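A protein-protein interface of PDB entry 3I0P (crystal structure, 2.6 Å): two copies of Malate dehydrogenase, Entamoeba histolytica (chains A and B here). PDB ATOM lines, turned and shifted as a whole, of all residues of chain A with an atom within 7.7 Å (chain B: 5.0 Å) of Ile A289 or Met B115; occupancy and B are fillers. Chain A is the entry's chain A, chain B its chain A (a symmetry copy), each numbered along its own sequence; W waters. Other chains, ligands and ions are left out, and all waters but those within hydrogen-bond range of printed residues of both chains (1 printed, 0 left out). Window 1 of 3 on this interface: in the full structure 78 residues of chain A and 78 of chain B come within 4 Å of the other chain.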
ATOM      1  N   MET A 101      19.091  -4.515 -23.786  1.00  0.00           N
ATOM      2  CA  MET A 101      19.014  -5.969 -23.861  1.00  0.00           C
ATOM      3  C   MET A 101      20.340  -6.627 -23.468  1.00  0.00           C
ATOM      4  O   MET A 101      20.351  -7.579 -22.690  1.00  0.00           O
ATOM      5  CB  MET A 101      18.544  -6.430 -25.254  1.00  0.00           C
ATOM      6  CG  MET A 101      18.520  -7.946 -25.449  1.00  0.00           C
ATOM      7  SD  MET A 101      17.460  -8.870 -24.306  1.00  0.00           S
ATOM      8  CE  MET A 101      15.884  -8.828 -25.154  1.00  0.00           C
ATOM      9  N   ALA A 104      20.230  -6.583 -19.950  1.00  0.00           N
ATOM     10  CA  ALA A 104      19.337  -7.622 -19.440  1.00  0.00           C
ATOM     11  C   ALA A 104      19.954  -9.026 -19.534  1.00  0.00           C
ATOM     12  O   ALA A 104      19.745  -9.857 -18.648  1.00  0.00           O
ATOM     13  CB  ALA A 104      18.003  -7.572 -20.152  1.00  0.00           C
ATOM     14  N   ILE A 105      20.707  -9.282 -20.606  1.00  0.00           N
ATOM     15  CA  ILE A 105      21.407 -10.556 -20.798  1.00  0.00           C
ATOM     16  C   ILE A 105      22.473 -10.753 -19.721  1.00  0.00           C
ATOM     17  O   ILE A 105      22.564 -11.816 -19.096  1.00  0.00           O
ATOM     18  CB  ILE A 105      22.066 -10.640 -22.199  1.00  0.00           C
ATOM     19  CG1 ILE A 105      21.004 -10.783 -23.288  1.00  0.00           C
ATOM     20  CG2 ILE A 105      23.054 -11.802 -22.276  1.00  0.00           C
ATOM     21  CD1 ILE A 105      21.505 -10.435 -24.685  1.00  0.00           C
ATOM     22  N   ALA A 108      21.012 -11.644 -16.604  1.00  0.00           N
ATOM     23  CA  ALA A 108      20.440 -12.987 -16.620  1.00  0.00           C
ATOM     24  C   ALA A 108      21.539 -14.012 -16.391  1.00  0.00           C
ATOM     25  O   ALA A 108      21.348 -14.969 -15.648  1.00  0.00           O
ATOM     26  CB  ALA A 108      19.688 -13.264 -17.920  1.00  0.00           C
ATOM     27  N   LYS A 109      22.697 -13.778 -17.011  1.00  0.00           N
ATOM     28  CA  LYS A 109      23.862 -14.649 -16.872  1.00  0.00           C
ATOM     29  C   LYS A 109      24.370 -14.720 -15.436  1.00  0.00           C
ATOM     30  O   LYS A 109      24.841 -15.766 -14.986  1.00  0.00           O
ATOM     31  CB  LYS A 109      24.983 -14.186 -17.796  1.00  0.00           C
ATOM     32  CG  LYS A 109      24.693 -14.375 -19.278  1.00  0.00           C
ATOM     33  CD  LYS A 109      24.663 -15.837 -19.657  1.00  0.00           C
ATOM     34  CE  LYS A 109      25.038 -16.011 -21.106  1.00  0.00           C
ATOM     35  NZ  LYS A 109      24.863 -17.425 -21.512  1.00  0.00           N
ATOM     36  N   GLY A 112      20.157 -15.290 -13.374  1.00  0.00           N
ATOM     37  CA  GLY A 112      19.137 -16.169 -13.949  1.00  0.00           C
ATOM     38  C   GLY A 112      18.171 -15.420 -14.845  1.00  0.00           C
ATOM     39  O   GLY A 112      17.740 -15.933 -15.880  1.00  0.00           O
ATOM     40  N   MET A 113      17.833 -14.196 -14.447  1.00  0.00           N
ATOM     41  CA  MET A 113      16.922 -13.361 -15.215  1.00  0.00           C
ATOM     42  C   MET A 113      17.314 -11.894 -15.195  1.00  0.00           C
ATOM     43  O   MET A 113      17.988 -11.435 -14.273  1.00  0.00           O
ATOM     44  CB  MET A 113      15.499 -13.525 -14.690  1.00  0.00           C
ATOM     45  CG  MET A 113      14.959 -14.916 -14.897  1.00  0.00           C
ATOM     46  SD  MET A 113      13.398 -15.093 -14.081  1.00  0.00           S
ATOM     47  CE  MET A 113      12.288 -14.436 -15.337  1.00  0.00           C
ATOM     48  N   GLY A 114      16.875 -11.166 -16.216  1.00  0.00           N
ATOM     49  CA  GLY A 114      17.154  -9.752 -16.327  1.00  0.00           C
ATOM     50  C   GLY A 114      16.041  -9.044 -17.062  1.00  0.00           C
ATOM     51  O   GLY A 114      15.471  -9.591 -18.021  1.00  0.00           O
ATOM     52  N   MET A 115      15.720  -7.833 -16.606  1.00  0.00           N
ATOM     53  CA  MET A 115      14.749  -6.978 -17.281  1.00  0.00           C
ATOM     54  C   MET A 115      15.192  -5.527 -17.264  1.00  0.00           C
ATOM     55  O   MET A 115      15.476  -4.954 -16.207  1.00  0.00           O
ATOM     56  CB  MET A 115      13.355  -7.104 -16.668  1.00  0.00           C
ATOM     57  CG  MET A 115      12.320  -6.226 -17.358  1.00  0.00           C
ATOM     58  SD  MET A 115      10.631  -6.769 -17.061  1.00  0.00           S
ATOM     59  CE  MET A 115       9.722  -5.546 -17.999  1.00  0.00           C
ATOM     60  N   ALA A 134      19.478 -11.983 -27.466  1.00  0.00           N
ATOM     61  CA  ALA A 134      19.296 -12.858 -26.318  1.00  0.00           C
ATOM     62  C   ALA A 134      19.470 -14.335 -26.680  1.00  0.00           C
ATOM     63  O   ALA A 134      20.142 -15.071 -25.957  1.00  0.00           O
ATOM     64  CB  ALA A 134      17.946 -12.610 -25.671  1.00  0.00           C
ATOM     65  N   ALA A 135      18.888 -14.754 -27.803  1.00  0.00           N
ATOM     66  CA  ALA A 135      18.998 -16.141 -28.261  1.00  0.00           C
ATOM     67  C   ALA A 135      20.444 -16.568 -28.591  1.00  0.00           C
ATOM     68  O   ALA A 135      20.827 -17.730 -28.368  1.00  0.00           O
ATOM     69  CB  ALA A 135      18.078 -16.385 -29.429  1.00  0.00           C
ATOM     70  N   GLU A 137      23.098 -15.590 -27.030  1.00  0.00           N
ATOM     71  CA  GLU A 137      23.741 -15.809 -25.728  1.00  0.00           C
ATOM     72  C   GLU A 137      23.103 -16.938 -24.909  1.00  0.00           C
ATOM     73  O   GLU A 137      23.359 -17.044 -23.707  1.00  0.00           O
ATOM     74  CB  GLU A 137      23.716 -14.522 -24.878  1.00  0.00           C
ATOM     75  CG  GLU A 137      24.481 -13.331 -25.442  1.00  0.00           C
ATOM     76  CD  GLU A 137      25.883 -13.701 -25.859  1.00  0.00           C
ATOM     77  OE1 GLU A 137      26.617 -14.281 -25.024  1.00  0.00           O
ATOM     78  OE2 GLU A 137      26.240 -13.430 -27.028  1.00  0.00           O
ATOM     79  N   GLY A 138      22.264 -17.760 -25.535  1.00  0.00           N
ATOM     80  CA  GLY A 138      21.616 -18.869 -24.828  1.00  0.00           C
ATOM     81  C   GLY A 138      20.519 -18.462 -23.851  1.00  0.00           C
ATOM     82  O   GLY A 138      20.192 -19.206 -22.920  1.00  0.00           O
ATOM     83  N   CYS A 139      19.943 -17.281 -24.068  1.00  0.00           N
ATOM     84  CA  CYS A 139      18.800 -16.815 -23.298  1.00  0.00           C
ATOM     85  C   CYS A 139      17.535 -16.763 -24.155  1.00  0.00           C
ATOM     86  O   CYS A 139      17.603 -16.558 -25.369  1.00  0.00           O
ATOM     87  CB  CYS A 139      19.067 -15.418 -22.775  1.00  0.00           C
ATOM     88  SG  CYS A 139      20.387 -15.279 -21.589  1.00  0.00           S
ATOM     89  N   ILE A 140      16.385 -16.964 -23.511  1.00  0.00           N
ATOM     90  CA  ILE A 140      15.099 -16.621 -24.098  1.00  0.00           C
ATOM     91  C   ILE A 140      15.027 -15.107 -24.024  1.00  0.00           C
ATOM     92  O   ILE A 140      15.277 -14.542 -22.964  1.00  0.00           O
ATOM     93  CB  ILE A 140      13.929 -17.242 -23.300  1.00  0.00           C
ATOM     94  CG1 ILE A 140      13.910 -18.768 -23.473  1.00  0.00           C
ATOM     95  CG2 ILE A 140      12.592 -16.657 -23.739  1.00  0.00           C
ATOM     96  CD1 ILE A 140      13.295 -19.549 -22.295  1.00  0.00           C
ATOM     97  N   GLY A 141      14.711 -14.452 -25.139  1.00  0.00           N
ATOM     98  CA  GLY A 141      14.581 -12.995 -25.162  1.00  0.00           C
ATOM     99  C   GLY A 141      13.204 -12.500 -25.556  1.00  0.00           C
ATOM    100  O   GLY A 141      12.692 -12.831 -26.624  1.00  0.00           O
ATOM    101  N   ILE A 142      12.604 -11.704 -24.686  1.00  0.00           N
ATOM    102  CA  ILE A 142      11.269 -11.165 -24.911  1.00  0.00           C
ATOM    103  C   ILE A 142      11.368  -9.649 -24.839  1.00  0.00           C
ATOM    104  O   ILE A 142      11.969  -9.103 -23.909  1.00  0.00           O
ATOM    105  CB  ILE A 142      10.246 -11.688 -23.859  1.00  0.00           C
ATOM    106  CG1 ILE A 142      10.183 -13.226 -23.880  1.00  0.00           C
ATOM    107  CG2 ILE A 142       8.870 -11.058 -24.090  1.00  0.00           C
ATOM    108  CD1 ILE A 142       9.450 -13.856 -22.697  1.00  0.00           C
ATOM    109  N   GLY A 169      12.633 -14.357 -28.834  1.00  0.00           N
ATOM    110  CA  GLY A 169      13.752 -15.121 -29.397  1.00  0.00           C
ATOM    111  C   GLY A 169      14.118 -16.292 -28.505  1.00  0.00           C
ATOM    112  O   GLY A 169      14.346 -16.121 -27.310  1.00  0.00           O
ATOM    113  N   PRO A 171      16.563 -19.912 -28.232  1.00  0.00           N
ATOM    114  CA  PRO A 171      17.622 -20.753 -28.800  1.00  0.00           C
ATOM    115  C   PRO A 171      17.074 -22.047 -29.421  1.00  0.00           C
ATOM    116  O   PRO A 171      16.109 -22.635 -28.907  1.00  0.00           O
ATOM    117  CB  PRO A 171      18.508 -21.060 -27.594  1.00  0.00           C
ATOM    118  CG  PRO A 171      18.299 -19.921 -26.678  1.00  0.00           C
ATOM    119  CD  PRO A 171      16.860 -19.525 -26.840  1.00  0.00           C
ATOM    120  N   ILE A 287      13.459  -8.376 -21.864  1.00  0.00           N
ATOM    121  CA  ILE A 287      13.549  -9.450 -20.887  1.00  0.00           C
ATOM    122  C   ILE A 287      14.493 -10.528 -21.401  1.00  0.00           C
ATOM    123  O   ILE A 287      14.411 -10.922 -22.557  1.00  0.00           O
ATOM    124  CB  ILE A 287      12.160 -10.078 -20.599  1.00  0.00           C
ATOM    125  CG1 ILE A 287      11.201  -9.046 -20.009  1.00  0.00           C
ATOM    126  CG2 ILE A 287      12.270 -11.310 -19.670  1.00  0.00           C
ATOM    127  CD1 ILE A 287       9.830  -9.622 -19.705  1.00  0.00           C
ATOM    128  N   ALA A 288      15.384 -10.997 -20.532  1.00  0.00           N
ATOM    129  CA  ALA A 288      16.271 -12.117 -20.845  1.00  0.00           C
ATOM    130  C   ALA A 288      16.199 -13.198 -19.756  1.00  0.00           C
ATOM    131  O   ALA A 288      16.272 -12.904 -18.562  1.00  0.00           O
ATOM    132  CB  ALA A 288      17.685 -11.627 -21.017  1.00  0.00           C
ATOM    133  N   ILE A 289      16.039 -14.445 -20.182  1.00  0.00           N
ATOM    134  CA  ILE A 289      15.929 -15.578 -19.272  1.00  0.00           C
ATOM    135  C   ILE A 289      17.054 -16.558 -19.583  1.00  0.00           C
ATOM    136  O   ILE A 289      17.156 -17.057 -20.702  1.00  0.00           O
ATOM    137  CB  ILE A 289      14.565 -16.304 -19.422  1.00  0.00           C
ATOM    138  CG1 ILE A 289      13.425 -15.385 -18.999  1.00  0.00           C
ATOM    139  CG2 ILE A 289      14.550 -17.625 -18.638  1.00  0.00           C
ATOM    140  CD1 ILE A 289      12.118 -15.760 -19.602  1.00  0.00           C
ATOM    141  N   ASN A 290      17.889 -16.831 -18.586  1.00  0.00           N
ATOM    142  CA  ASN A 290      19.035 -17.705 -18.769  1.00  0.00           C
ATOM    143  C   ASN A 290      18.627 -19.169 -18.722  1.00  0.00           C
ATOM    144  O   ASN A 290      18.322 -19.702 -17.656  1.00  0.00           O
ATOM    145  CB  ASN A 290      20.102 -17.407 -17.714  1.00  0.00           C
ATOM    146  CG  ASN A 290      21.403 -18.141 -17.969  1.00  0.00           C
ATOM    147  OD1 ASN A 290      21.616 -18.719 -19.038  1.00  0.00           O
ATOM    148  ND2 ASN A 290      22.292 -18.110 -16.984  1.00  0.00           N
ATOM    149  N   VAL A 291      18.632 -19.803 -19.890  1.00  0.00           N
ATOM    150  CA  VAL A 291      18.235 -21.200 -20.043  1.00  0.00           C
ATOM    151  C   VAL A 291      19.018 -22.169 -19.129  1.00  0.00           C
ATOM    152  O   VAL A 291      18.411 -23.022 -18.450  1.00  0.00           O
ATOM    153  CB  VAL A 291      18.329 -21.643 -21.529  1.00  0.00           C
ATOM    154  CG1 VAL A 291      18.314 -23.172 -21.660  1.00  0.00           C
ATOM    155  CG2 VAL A 291      17.214 -21.003 -22.354  1.00  0.00           C
ATOM    156  N   GLU A 292      20.347 -22.020 -19.089  1.00  0.00           N
ATOM    157  CA  GLU A 292      21.197 -22.971 -18.373  1.00  0.00           C
ATOM    158  C   GLU A 292      20.904 -23.044 -16.857  1.00  0.00           C
ATOM    159  O   GLU A 292      21.288 -24.010 -16.199  1.00  0.00           O
ATOM    160  CB  GLU A 292      22.694 -22.774 -18.709  1.00  0.00           C
ATOM    161  CG  GLU A 292      23.408 -21.622 -17.972  1.00  0.00           C
ATOM    162  CD  GLU A 292      24.745 -21.200 -18.633  1.00  0.00           C
ATOM    163  OE1 GLU A 292      25.288 -21.995 -19.449  1.00  0.00           O
ATOM    164  OE2 GLU A 292      25.239 -20.070 -18.339  1.00  0.00           O
ATOM    165  N   CYS A 293      20.200 -22.041 -16.325  1.00  0.00           N
ATOM    166  CA  CYS A 293      19.671 -22.087 -14.948  1.00  0.00           C
ATOM    167  C   CYS A 293      18.613 -23.179 -14.740  1.00  0.00           C
ATOM    168  O   CYS A 293      18.377 -23.613 -13.606  1.00  0.00           O
ATOM    169  CB  CYS A 293      19.071 -20.743 -14.555  1.00  0.00           C
ATOM    170  SG  CYS A 293      20.284 -19.446 -14.285  1.00  0.00           S
ATOM    171  N   PHE A 294      17.991 -23.614 -15.840  1.00  0.00           N
ATOM    172  CA  PHE A 294      16.891 -24.577 -15.815  1.00  0.00           C
ATOM    173  C   PHE A 294      17.309 -25.947 -16.299  1.00  0.00           C
ATOM    174  O   PHE A 294      17.020 -26.953 -15.657  1.00  0.00           O
ATOM    175  CB  PHE A 294      15.740 -24.104 -16.714  1.00  0.00           C
ATOM    176  CG  PHE A 294      15.053 -22.875 -16.221  1.00  0.00           C
ATOM    177  CD1 PHE A 294      14.056 -22.965 -15.246  1.00  0.00           C
ATOM    178  CD2 PHE A 294      15.393 -21.624 -16.735  1.00  0.00           C
ATOM    179  CE1 PHE A 294      13.410 -21.821 -14.784  1.00  0.00           C
ATOM    180  CE2 PHE A 294      14.766 -20.479 -16.283  1.00  0.00           C
ATOM    181  CZ  PHE A 294      13.763 -20.575 -15.308  1.00  0.00           C
ATOM    182  N   PHE A 300      18.103 -28.409 -24.269  1.00  0.00           N
ATOM    183  CA  PHE A 300      17.010 -27.462 -24.526  1.00  0.00           C
ATOM    184  C   PHE A 300      16.875 -27.097 -26.006  1.00  0.00           C
ATOM    185  O   PHE A 300      15.765 -27.124 -26.552  1.00  0.00           O
ATOM    186  CB  PHE A 300      17.191 -26.191 -23.689  1.00  0.00           C
ATOM    187  CG  PHE A 300      16.255 -25.064 -24.069  1.00  0.00           C
ATOM    188  CD1 PHE A 300      15.072 -24.853 -23.357  1.00  0.00           C
ATOM    189  CD2 PHE A 300      16.560 -24.208 -25.128  1.00  0.00           C
ATOM    190  CE1 PHE A 300      14.209 -23.813 -23.694  1.00  0.00           C
ATOM    191  CE2 PHE A 300      15.695 -23.171 -25.476  1.00  0.00           C
ATOM    192  CZ  PHE A 300      14.517 -22.971 -24.754  1.00  0.00           C
ATOM    193  N   THR B  82      16.790 -16.915  -8.857  1.00  0.00           N
ATOM    194  CA  THR B  82      15.606 -16.355  -9.495  1.00  0.00           C
ATOM    195  C   THR B  82      14.782 -17.407 -10.220  1.00  0.00           C
ATOM    196  O   THR B  82      13.724 -17.094 -10.770  1.00  0.00           O
ATOM    197  CB  THR B  82      15.993 -15.278 -10.534  1.00  0.00           C
ATOM    198  OG1 THR B  82      16.909 -15.844 -11.484  1.00  0.00           O
ATOM    199  CG2 THR B  82      16.637 -14.072  -9.870  1.00  0.00           C
ATOM    200  N   THR B  83      15.267 -18.644 -10.244  1.00  0.00           N
ATOM    201  CA  THR B  83      14.613 -19.703 -11.026  1.00  0.00           C
ATOM    202  C   THR B  83      14.366 -20.974 -10.226  1.00  0.00           C
ATOM    203  O   THR B  83      14.899 -21.140  -9.122  1.00  0.00           O
ATOM    204  CB  THR B  83      15.430 -20.103 -12.283  1.00  0.00           C
ATOM    205  OG1 THR B  83      16.560 -20.896 -11.896  1.00  0.00           O
ATOM    206  CG2 THR B  83      15.883 -18.874 -13.073  1.00  0.00           C
ATOM    207  N   CYS B  84      13.559 -21.868 -10.800  1.00  0.00           N
ATOM    208  CA  CYS B  84      13.369 -23.201 -10.249  1.00  0.00           C
ATOM    209  C   CYS B  84      12.705 -24.152 -11.251  1.00  0.00           C
ATOM    210  O   CYS B  84      11.868 -23.727 -12.055  1.00  0.00           O
ATOM    211  CB  CYS B  84      12.567 -23.144  -8.945  1.00  0.00           C
ATOM    212  SG  CYS B  84      12.541 -24.711  -8.049  1.00  0.00           S
ATOM    213  N   ALA B 104       7.788 -18.220  -7.391  1.00  0.00           N
ATOM    214  CA  ALA B 104       8.282 -17.195  -8.307  1.00  0.00           C
ATOM    215  C   ALA B 104       8.129 -15.775  -7.740  1.00  0.00           C
ATOM    216  O   ALA B 104       8.990 -14.922  -7.958  1.00  0.00           O
ATOM    217  CB  ALA B 104       7.602 -17.313  -9.653  1.00  0.00           C
ATOM    218  N   MET B 113      13.088 -10.510  -9.925  1.00  0.00           N
ATOM    219  CA  MET B 113      12.369 -11.399 -10.824  1.00  0.00           C
ATOM    220  C   MET B 113      12.428 -12.851 -10.382  1.00  0.00           C
ATOM    221  O   MET B 113      13.350 -13.257  -9.674  1.00  0.00           O
ATOM    222  CB  MET B 113      12.920 -11.265 -12.240  1.00  0.00           C
ATOM    223  CG  MET B 113      12.679  -9.900 -12.831  1.00  0.00           C
ATOM    224  SD  MET B 113      13.524  -9.748 -14.379  1.00  0.00           S
ATOM    225  CE  MET B 113      12.314 -10.483 -15.493  1.00  0.00           C
ATOM    226  N   GLY B 114      11.442 -13.628 -10.818  1.00  0.00           N
ATOM    227  CA  GLY B 114      11.372 -15.035 -10.494  1.00  0.00           C
ATOM    228  C   GLY B 114      10.684 -15.802 -11.598  1.00  0.00           C
ATOM    229  O   GLY B 114       9.722 -15.308 -12.206  1.00  0.00           O
ATOM    230  N   MET B 115      11.188 -17.007 -11.869  1.00  0.00           N
ATOM    231  CA  MET B 115      10.563 -17.916 -12.824  1.00  0.00           C
ATOM    232  C   MET B 115      10.618 -19.351 -12.332  1.00  0.00           C
ATOM    233  O   MET B 115      11.687 -19.879 -12.007  1.00  0.00           O
ATOM    234  CB  MET B 115      11.202 -17.816 -14.208  1.00  0.00           C
ATOM    235  CG  MET B 115      10.565 -18.751 -15.227  1.00  0.00           C
ATOM    236  SD  MET B 115      10.880 -18.254 -16.927  1.00  0.00           S
ATOM    237  CE  MET B 115      10.004 -19.537 -17.814  1.00  0.00           C
ATOM    238  N   VAL B 116       9.457 -19.986 -12.283  1.00  0.00           N
ATOM    239  CA  VAL B 116       9.390 -21.367 -11.869  1.00  0.00           C
ATOM    240  C   VAL B 116       8.696 -22.135 -12.956  1.00  0.00           C
ATOM    241  O   VAL B 116       7.643 -21.708 -13.434  1.00  0.00           O
ATOM    242  CB  VAL B 116       8.661 -21.516 -10.529  1.00  0.00           C
ATOM    243  CG1 VAL B 116       8.389 -22.969 -10.229  1.00  0.00           C
ATOM    244  CG2 VAL B 116       9.500 -20.899  -9.420  1.00  0.00           C
ATOM    245  N   VAL B 117       9.299 -23.245 -13.376  1.00  0.00           N
ATOM    246  CA  VAL B 117       8.673 -24.119 -14.376  1.00  0.00           C
ATOM    247  C   VAL B 117       8.323 -25.485 -13.780  1.00  0.00           C
ATOM    248  O   VAL B 117       8.926 -25.915 -12.794  1.00  0.00           O
ATOM    249  CB  VAL B 117       9.526 -24.258 -15.675  1.00  0.00           C
ATOM    250  CG1 VAL B 117       9.646 -22.910 -16.370  1.00  0.00           C
ATOM    251  CG2 VAL B 117      10.904 -24.839 -15.375  1.00  0.00           C
ATOM    252  N   MET B 257       7.895 -22.658 -23.426  1.00  0.00           N
ATOM    253  CA  MET B 257       8.012 -22.192 -22.044  1.00  0.00           C
ATOM    254  C   MET B 257       7.502 -23.239 -21.057  1.00  0.00           C
ATOM    255  O   MET B 257       8.029 -23.365 -19.953  1.00  0.00           O
ATOM    256  CB  MET B 257       7.232 -20.878 -21.839  1.00  0.00           C
ATOM    257  CG  MET B 257       7.712 -19.699 -22.676  1.00  0.00           C
ATOM    258  SD  MET B 257       9.296 -19.075 -22.113  1.00  0.00           S
ATOM    259  CE  MET B 257       8.792 -17.903 -20.850  1.00  0.00           C
ATOM    260  N   LEU B 261      11.865 -26.050 -20.676  1.00  0.00           N
ATOM    261  CA  LEU B 261      12.671 -25.697 -19.519  1.00  0.00           C
ATOM    262  C   LEU B 261      12.555 -26.730 -18.393  1.00  0.00           C
ATOM    263  O   LEU B 261      13.519 -26.989 -17.692  1.00  0.00           O
ATOM    264  CB  LEU B 261      12.351 -24.272 -19.049  1.00  0.00           C
ATOM    265  CG  LEU B 261      12.738 -23.148 -20.032  1.00  0.00           C
ATOM    266  CD1 LEU B 261      12.010 -21.851 -19.730  1.00  0.00           C
ATOM    267  CD2 LEU B 261      14.244 -22.910 -20.077  1.00  0.00           C
ATOM    268  N   PHE B 285       4.505 -22.877 -16.801  1.00  0.00           N
ATOM    269  CA  PHE B 285       5.507 -21.879 -16.406  1.00  0.00           C
ATOM    270  C   PHE B 285       4.856 -20.712 -15.677  1.00  0.00           C
ATOM    271  O   PHE B 285       3.682 -20.396 -15.921  1.00  0.00           O
ATOM    272  CB  PHE B 285       6.308 -21.360 -17.603  1.00  0.00           C
ATOM    273  CG  PHE B 285       5.522 -20.486 -18.540  1.00  0.00           C
ATOM    274  CD1 PHE B 285       5.595 -19.102 -18.439  1.00  0.00           C
ATOM    275  CD2 PHE B 285       4.725 -21.049 -19.533  1.00  0.00           C
ATOM    276  CE1 PHE B 285       4.875 -18.275 -19.312  1.00  0.00           C
ATOM    277  CE2 PHE B 285       3.999 -20.236 -20.414  1.00  0.00           C
ATOM    278  CZ  PHE B 285       4.076 -18.851 -20.309  1.00  0.00           C
ATOM    279  N   PHE B 286       5.629 -20.081 -14.792  1.00  0.00           N
ATOM    280  CA  PHE B 286       5.151 -18.970 -13.970  1.00  0.00           C
ATOM    281  C   PHE B 286       6.252 -17.939 -13.806  1.00  0.00           C
ATOM    282  O   PHE B 286       7.334 -18.253 -13.292  1.00  0.00           O
ATOM    283  CB  PHE B 286       4.694 -19.468 -12.597  1.00  0.00           C
ATOM    284  CG  PHE B 286       3.705 -20.587 -12.666  1.00  0.00           C
ATOM    285  CD1 PHE B 286       2.357 -20.325 -12.881  1.00  0.00           C
ATOM    286  CD2 PHE B 286       4.122 -21.907 -12.532  1.00  0.00           C
ATOM    287  CE1 PHE B 286       1.433 -21.349 -12.962  1.00  0.00           C
ATOM    288  CE2 PHE B 286       3.206 -22.941 -12.603  1.00  0.00           C
ATOM    289  CZ  PHE B 286       1.849 -22.658 -12.829  1.00  0.00           C
ATOM    290  N   ILE B 287       5.966 -16.717 -14.257  1.00  0.00           N
ATOM    291  CA  ILE B 287       6.905 -15.608 -14.183  1.00  0.00           C
ATOM    292  C   ILE B 287       6.335 -14.517 -13.287  1.00  0.00           C
ATOM    293  O   ILE B 287       5.168 -14.166 -13.406  1.00  0.00           O
ATOM    294  CB  ILE B 287       7.202 -15.017 -15.586  1.00  0.00           C
ATOM    295  CG1 ILE B 287       7.848 -16.060 -16.496  1.00  0.00           C
ATOM    296  CG2 ILE B 287       8.088 -13.751 -15.497  1.00  0.00           C
ATOM    297  CD1 ILE B 287       8.163 -15.519 -17.879  1.00  0.00           C
HETATM  298  O   HOH W   1      16.262 -23.510 -11.904  1.00  0.00           O
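The side-chain sulfur of Met A113 lies close to the backbone NH of Met B115 (3.7 Å). The side-chain sulfur (SD) of Met B113 sits close to the backbone NH (N) of Met A115.
The backbone carbonyl oxygen of Gly A112 is in hydrogen-bond range of the backbone NH of Asn A290 (2.9 Å). The backbone NH (N) of Ala A288 is in hydrogen-bond range of the backbone carbonyl oxygen (O) of Gly A114 (2.9 Å). The backbone carbonyl oxygen (O) of Ile A140 lies within hydrogen-bond range of the backbone NH (N) of Ile A289 (2.9 Å). The side-chain amide nitrogen (ND2) of Asn A290 is in hydrogen-bond range of the side-chain sulfur (SG) of Cys A293, 3.6 Å away. The backbone carbonyl oxygen (O) of Met B115 lies within hydrogen-bond range of the backbone NH (N) of Cys B84 (3.0 Å). N of Val B117 lies within hydrogen-bond range of O of Cys B84, 2.9 Å away.
Among the printed residues, pairs that only touch across the chains: Gly A112 with Thr B82 (3.3 Å), Met A113 with Thr B82 (3.5 Å), Met A113 with Met B113 (3.96 Å), Met A113 with Gly B114 (3.7 Å), Gly A114 with Met B113 (3.7 Å), Ile A140 with Leu B261 (3.7 Å), Ile A289 with Met B115 (3.9 Å), Cys A293 with Thr B83 (3.7 Å), Phe A294 with Thr B83 (3.5 Å), Phe A294 with Cys B84 (3.7 Å), Phe A294 with Met B115 (3.7 Å), Phe A294 with Val B117 (3.7 Å), Phe A294 with Leu B261 (3.8 Å) and Phe A300 with Leu B261 (3.7 Å).
Ile A289 touches just one residue of chain B: Met B115 (3.9 Å). Of chain A, only Met A113, Ile A289 and Phe A294 come within 4 Å of Met B115. Gly B114 touches just one residue of chain A: Met A113. Of the printed residues of chain B, Phe A300 touches Leu B261. Of the printed residues of chain B, Gly A112 touches Thr B82 (3.3 Å). Of the printed residues of chain B, Met A115 touches Met B113 (3.5 Å). Of the printed residues of chain B, Phe A294 touches Thr B83 (3.5 Å), Cys B84 (3.7 Å), Met B115 (3.7 Å), Val B117 (3.7 Å) and Leu B261 (3.8 Å). Phe B285 touches none of the printed residues of chain A.
Of the 28 printed residues of chain A, 9 touch a printed residue of chain B.
Met A113 touches its own counterpart, Met B113. Met A113 touches Gly B114, and with the chains exchanged Gly A114 touches Met B113. Met A113 touches Met B115, and with the chains exchanged Met A115 touches Met B113.
Water W1 lies within hydrogen-bond range of OG1 of Thr B83 (2.6 Å), O of Cys A293 (2.7 Å) and N of Cys B84 (3.3 Å).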
